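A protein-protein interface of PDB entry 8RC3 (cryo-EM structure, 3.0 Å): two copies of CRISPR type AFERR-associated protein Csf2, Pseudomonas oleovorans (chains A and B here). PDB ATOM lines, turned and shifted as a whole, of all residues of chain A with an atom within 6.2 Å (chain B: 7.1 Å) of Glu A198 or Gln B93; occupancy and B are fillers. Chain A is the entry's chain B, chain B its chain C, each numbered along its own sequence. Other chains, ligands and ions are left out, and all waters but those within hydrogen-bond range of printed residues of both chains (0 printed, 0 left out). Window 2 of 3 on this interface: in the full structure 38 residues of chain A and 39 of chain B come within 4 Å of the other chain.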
ATOM      1  N   ALA A 194     -12.344 -20.555  30.241  1.00  0.00           N
ATOM      2  CA  ALA A 194     -13.521 -19.900  29.693  1.00  0.00           C
ATOM      3  C   ALA A 194     -14.040 -20.573  28.431  1.00  0.00           C
ATOM      4  O   ALA A 194     -15.013 -20.089  27.846  1.00  0.00           O
ATOM      5  CB  ALA A 194     -13.218 -18.428  29.401  1.00  0.00           C
ATOM      6  N   ALA A 195     -13.411 -21.664  27.992  1.00  0.00           N
ATOM      7  CA  ALA A 195     -13.862 -22.336  26.778  1.00  0.00           C
ATOM      8  C   ALA A 195     -15.218 -23.001  26.980  1.00  0.00           C
ATOM      9  O   ALA A 195     -16.038 -23.039  26.057  1.00  0.00           O
ATOM     10  CB  ALA A 195     -12.824 -23.362  26.329  1.00  0.00           C
ATOM     11  N   VAL A 196     -15.468 -23.537  28.177  1.00  0.00           N
ATOM     12  CA  VAL A 196     -16.754 -24.162  28.455  1.00  0.00           C
ATOM     13  C   VAL A 196     -17.864 -23.127  28.564  1.00  0.00           C
ATOM     14  O   VAL A 196     -19.041 -23.464  28.410  1.00  0.00           O
ATOM     15  CB  VAL A 196     -16.666 -25.017  29.734  1.00  0.00           C
ATOM     16  CG1 VAL A 196     -16.599 -24.132  30.963  1.00  0.00           C
ATOM     17  CG2 VAL A 196     -17.833 -25.987  29.821  1.00  0.00           C
ATOM     18  N   ILE A 197     -17.520 -21.870  28.816  1.00  0.00           N
ATOM     19  CA  ILE A 197     -18.518 -20.814  28.941  1.00  0.00           C
ATOM     20  C   ILE A 197     -18.959 -20.375  27.555  1.00  0.00           C
ATOM     21  O   ILE A 197     -18.128 -20.049  26.699  1.00  0.00           O
ATOM     22  CB  ILE A 197     -17.956 -19.629  29.738  1.00  0.00           C
ATOM     23  CG1 ILE A 197     -17.609 -20.054  31.160  1.00  0.00           C
ATOM     24  CG2 ILE A 197     -18.948 -18.491  29.756  1.00  0.00           C
ATOM     25  CD1 ILE A 197     -17.011 -18.947  31.982  1.00  0.00           C
ATOM     26  N   GLU A 198     -20.270 -20.370  27.325  1.00  0.00           N
ATOM     27  CA  GLU A 198     -20.803 -19.862  26.071  1.00  0.00           C
ATOM     28  C   GLU A 198     -20.455 -18.388  25.929  1.00  0.00           C
ATOM     29  O   GLU A 198     -20.652 -17.600  26.857  1.00  0.00           O
ATOM     30  CB  GLU A 198     -22.315 -20.063  26.021  1.00  0.00           C
ATOM     31  CG  GLU A 198     -22.983 -19.476  24.795  1.00  0.00           C
ATOM     32  CD  GLU A 198     -24.478 -19.722  24.776  1.00  0.00           C
ATOM     33  OE1 GLU A 198     -24.898 -20.860  25.071  1.00  0.00           O
ATOM     34  OE2 GLU A 198     -25.234 -18.777  24.472  1.00  0.00           O
ATOM     35  N   GLY A 199     -19.936 -18.018  24.766  1.00  0.00           N
ATOM     36  CA  GLY A 199     -19.393 -16.689  24.539  1.00  0.00           C
ATOM     37  C   GLY A 199     -17.936 -16.583  24.936  1.00  0.00           C
ATOM     38  O   GLY A 199     -17.133 -15.994  24.210  1.00  0.00           O
ATOM     39  N   GLY A 200     -17.581 -17.148  26.087  1.00  0.00           N
ATOM     40  CA  GLY A 200     -16.194 -17.248  26.494  1.00  0.00           C
ATOM     41  C   GLY A 200     -15.603 -15.983  27.076  1.00  0.00           C
ATOM     42  O   GLY A 200     -16.089 -15.459  28.085  1.00  0.00           O
ATOM     43  N   ALA A 203     -18.053 -13.054  27.279  1.00  0.00           N
ATOM     44  CA  ALA A 203     -18.989 -13.179  28.391  1.00  0.00           C
ATOM     45  C   ALA A 203     -18.308 -12.887  29.720  1.00  0.00           C
ATOM     46  O   ALA A 203     -18.881 -12.213  30.585  1.00  0.00           O
ATOM     47  CB  ALA A 203     -19.609 -14.575  28.402  1.00  0.00           C
ATOM     48  N   LEU B  87     -18.059 -32.559  29.375  1.00  0.00           N
ATOM     49  CA  LEU B  87     -18.759 -31.558  28.579  1.00  0.00           C
ATOM     50  C   LEU B  87     -17.963 -31.163  27.341  1.00  0.00           C
ATOM     51  O   LEU B  87     -18.552 -30.886  26.292  1.00  0.00           O
ATOM     52  CB  LEU B  87     -19.055 -30.323  29.427  1.00  0.00           C
ATOM     53  CG  LEU B  87     -20.298 -30.358  30.316  1.00  0.00           C
ATOM     54  CD1 LEU B  87     -20.459 -29.042  31.054  1.00  0.00           C
ATOM     55  CD2 LEU B  87     -21.532 -30.658  29.493  1.00  0.00           C
ATOM     56  N   LYS B  90     -18.380 -33.374  24.033  1.00  0.00           N
ATOM     57  CA  LYS B  90     -19.567 -33.121  23.233  1.00  0.00           C
ATOM     58  C   LYS B  90     -19.666 -31.682  22.756  1.00  0.00           C
ATOM     59  O   LYS B  90     -20.644 -31.336  22.085  1.00  0.00           O
ATOM     60  CB  LYS B  90     -20.819 -33.479  24.032  1.00  0.00           C
ATOM     61  CG  LYS B  90     -20.641 -34.690  24.915  1.00  0.00           C
ATOM     62  CD  LYS B  90     -21.833 -34.896  25.819  1.00  0.00           C
ATOM     63  CE  LYS B  90     -21.735 -36.233  26.522  1.00  0.00           C
ATOM     64  NZ  LYS B  90     -20.369 -36.461  27.065  1.00  0.00           N
ATOM     65  N   SER B  91     -18.684 -30.842  23.084  1.00  0.00           N
ATOM     66  CA  SER B  91     -18.711 -29.419  22.747  1.00  0.00           C
ATOM     67  C   SER B  91     -19.979 -28.750  23.273  1.00  0.00           C
ATOM     68  O   SER B  91     -20.609 -27.944  22.586  1.00  0.00           O
ATOM     69  CB  SER B  91     -18.564 -29.203  21.240  1.00  0.00           C
ATOM     70  OG  SER B  91     -17.299 -29.653  20.786  1.00  0.00           O
ATOM     71  N   ALA B  92     -20.356 -29.089  24.502  1.00  0.00           N
ATOM     72  CA  ALA B  92     -21.493 -28.466  25.163  1.00  0.00           C
ATOM     73  C   ALA B  92     -21.000 -27.314  26.026  1.00  0.00           C
ATOM     74  O   ALA B  92     -20.104 -27.491  26.856  1.00  0.00           O
ATOM     75  CB  ALA B  92     -22.253 -29.485  26.013  1.00  0.00           C
ATOM     76  N   GLN B  93     -21.584 -26.139  25.825  1.00  0.00           N
ATOM     77  CA  GLN B  93     -21.116 -24.910  26.451  1.00  0.00           C
ATOM     78  C   GLN B  93     -22.133 -24.436  27.478  1.00  0.00           C
ATOM     79  O   GLN B  93     -23.310 -24.246  27.152  1.00  0.00           O
ATOM     80  CB  GLN B  93     -20.875 -23.826  25.401  1.00  0.00           C
ATOM     81  CG  GLN B  93     -19.428 -23.691  24.975  1.00  0.00           C
ATOM     82  CD  GLN B  93     -19.266 -22.834  23.742  1.00  0.00           C
ATOM     83  OE1 GLN B  93     -20.246 -22.442  23.111  1.00  0.00           O
ATOM     84  NE2 GLN B  93     -18.022 -22.528  23.394  1.00  0.00           N
ATOM     85  N   LEU B  94     -21.676 -24.242  28.711  1.00  0.00           N
ATOM     86  CA  LEU B  94     -22.506 -23.653  29.747  1.00  0.00           C
ATOM     87  C   LEU B  94     -22.600 -22.146  29.554  1.00  0.00           C
ATOM     88  O   LEU B  94     -21.656 -21.499  29.096  1.00  0.00           O
ATOM     89  CB  LEU B  94     -21.938 -23.954  31.131  1.00  0.00           C
ATOM     90  CG  LEU B  94     -21.854 -25.420  31.533  1.00  0.00           C
ATOM     91  CD1 LEU B  94     -21.329 -25.553  32.946  1.00  0.00           C
ATOM     92  CD2 LEU B  94     -23.211 -26.066  31.402  1.00  0.00           C
ATOM     93  N   SER B  95     -23.752 -21.590  29.909  1.00  0.00           N
ATOM     94  CA  SER B  95     -23.884 -20.146  29.942  1.00  0.00           C
ATOM     95  C   SER B  95     -23.097 -19.584  31.122  1.00  0.00           C
ATOM     96  O   SER B  95     -22.613 -20.318  31.988  1.00  0.00           O
ATOM     97  CB  SER B  95     -25.354 -19.745  30.030  1.00  0.00           C
ATOM     98  OG  SER B  95     -26.028 -20.509  31.013  1.00  0.00           O
ATOM     99  N   ILE B  96     -22.956 -18.259  31.147  1.00  0.00           N
ATOM    100  CA  ILE B  96     -22.202 -17.628  32.226  1.00  0.00           C
ATOM    101  C   ILE B  96     -22.900 -17.846  33.565  1.00  0.00           C
ATOM    102  O   ILE B  96     -22.255 -18.153  34.576  1.00  0.00           O
ATOM    103  CB  ILE B  96     -21.966 -16.136  31.912  1.00  0.00           C
ATOM    104  CG1 ILE B  96     -20.837 -15.578  32.776  1.00  0.00           C
ATOM    105  CG2 ILE B  96     -23.240 -15.308  32.041  1.00  0.00           C
ATOM    106  CD1 ILE B  96     -19.504 -16.205  32.498  1.00  0.00           C
ATOM    107  N   ALA B  98     -24.988 -20.362  34.249  1.00  0.00           N
ATOM    108  CA  ALA B  98     -24.878 -21.785  34.554  1.00  0.00           C
ATOM    109  C   ALA B  98     -23.496 -22.129  35.087  1.00  0.00           C
ATOM    110  O   ALA B  98     -23.365 -22.916  36.029  1.00  0.00           O
ATOM    111  CB  ALA B  98     -25.197 -22.614  33.313  1.00  0.00           C
ATOM    112  N   TYR B  99     -22.450 -21.546  34.498  1.00  0.00           N
ATOM    113  CA  TYR B  99     -21.098 -21.771  34.995  1.00  0.00           C
ATOM    114  C   TYR B  99     -20.941 -21.251  36.417  1.00  0.00           C
ATOM    115  O   TYR B  99     -20.362 -21.929  37.277  1.00  0.00           O
ATOM    116  CB  TYR B  99     -20.093 -21.103  34.060  1.00  0.00           C
ATOM    117  CG  TYR B  99     -18.648 -21.291  34.447  1.00  0.00           C
ATOM    118  CD1 TYR B  99     -18.012 -20.394  35.290  1.00  0.00           C
ATOM    119  CD2 TYR B  99     -17.913 -22.357  33.955  1.00  0.00           C
ATOM    120  CE1 TYR B  99     -16.694 -20.560  35.641  1.00  0.00           C
ATOM    121  CE2 TYR B  99     -16.594 -22.528  34.299  1.00  0.00           C
ATOM    122  CZ  TYR B  99     -15.990 -21.628  35.143  1.00  0.00           C
ATOM    123  OH  TYR B  99     -14.672 -21.797  35.491  1.00  0.00           O
ATOM    124  N   SER B 334     -25.609 -30.181  28.906  1.00  0.00           N
ATOM    125  CA  SER B 334     -25.675 -28.911  29.620  1.00  0.00           C
ATOM    126  C   SER B 334     -27.094 -28.492  29.975  1.00  0.00           C
ATOM    127  O   SER B 334     -27.260 -27.517  30.717  1.00  0.00           O
ATOM    128  CB  SER B 334     -25.018 -27.814  28.789  1.00  0.00           C
ATOM    129  OG  SER B 334     -25.511 -27.823  27.463  1.00  0.00           O
ATOM    130  N   GLU B 338     -28.302 -25.632  32.715  1.00  0.00           N
ATOM    131  CA  GLU B 338     -29.051 -24.442  32.320  1.00  0.00           C
ATOM    132  C   GLU B 338     -30.393 -24.369  33.035  1.00  0.00           C
ATOM    133  O   GLU B 338     -30.819 -23.291  33.462  1.00  0.00           O
ATOM    134  CB  GLU B 338     -29.248 -24.422  30.806  1.00  0.00           C
ATOM    135  CG  GLU B 338     -27.964 -24.556  30.007  1.00  0.00           C
ATOM    136  CD  GLU B 338     -27.317 -23.221  29.703  1.00  0.00           C
ATOM    137  OE1 GLU B 338     -27.277 -22.356  30.602  1.00  0.00           O
ATOM    138  OE2 GLU B 338     -26.848 -23.037  28.560  1.00  0.00           O
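No position is printed for both chains. Of the 9 pairs that touch across the chains among the printed residues, none has its exchanged pair printed and touching as well.
Of chain B, only Gln B93 (3.97 Å) and Leu B94 (2.5 Å) come within 4 Å of Glu A198. Of the printed residues of chain A, Ile B96 touches Ile A197 (3.6 Å). Printed residues of chain A within 4 Å of Tyr B99: Val A196 (3.7 Å) and Ile A197 (3.6 Å). Printed residues of chain B within 4 Å of Ile A197: Leu B94 (3.2 Å), Ile B96 (3.6 Å) and Tyr B99 (3.6 Å). Printed residues of chain A within 4 Å of Leu B94: Val A196 (2.8 Å), Ile A197 (3.2 Å) and Glu A198 (2.5 Å). Of the printed residues of chain B, Ala A195 touches Gln B93 (3.4 Å). Lys B90 touches none of the printed residues of chain A. The nearest residue of chain B that does not touch Glu A198 is Ser B95 (4.2 Å). The nearest printed residue of chain A that does not touch Ile B96 is Ala A203 (4.4 Å).
Of the 12 printed residues of chain B, 4 touch a printed residue of chain A. Hydrophobic or aromatic side chains of chain B that line the printed part of chain A: Ile B96 and Tyr B99.
O of Val A196 is in hydrogen-bond range of N of Leu B94 (2.8 Å). The backbone carbonyl oxygen of Ala A195 sits at hydrogen-bond distance from the side-chain amide nitrogen of Gln B93 (3.4 Å). O of Leu B94 lies within hydrogen-bond range of N of Glu A198 (2.5 Å).
Among the printed residues, pairs that only touch across the chains: Val A196 with Gln B93 (3.2 Å), Val A196 with Tyr B99 (3.7 Å), Ile A197 with Leu B94 (3.2 Å), Ile A197 with Ile B96 (3.6 Å), Ile A197 with Tyr B99 (3.6 Å) and Glu A198 with Gln B93 (3.97 Å).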
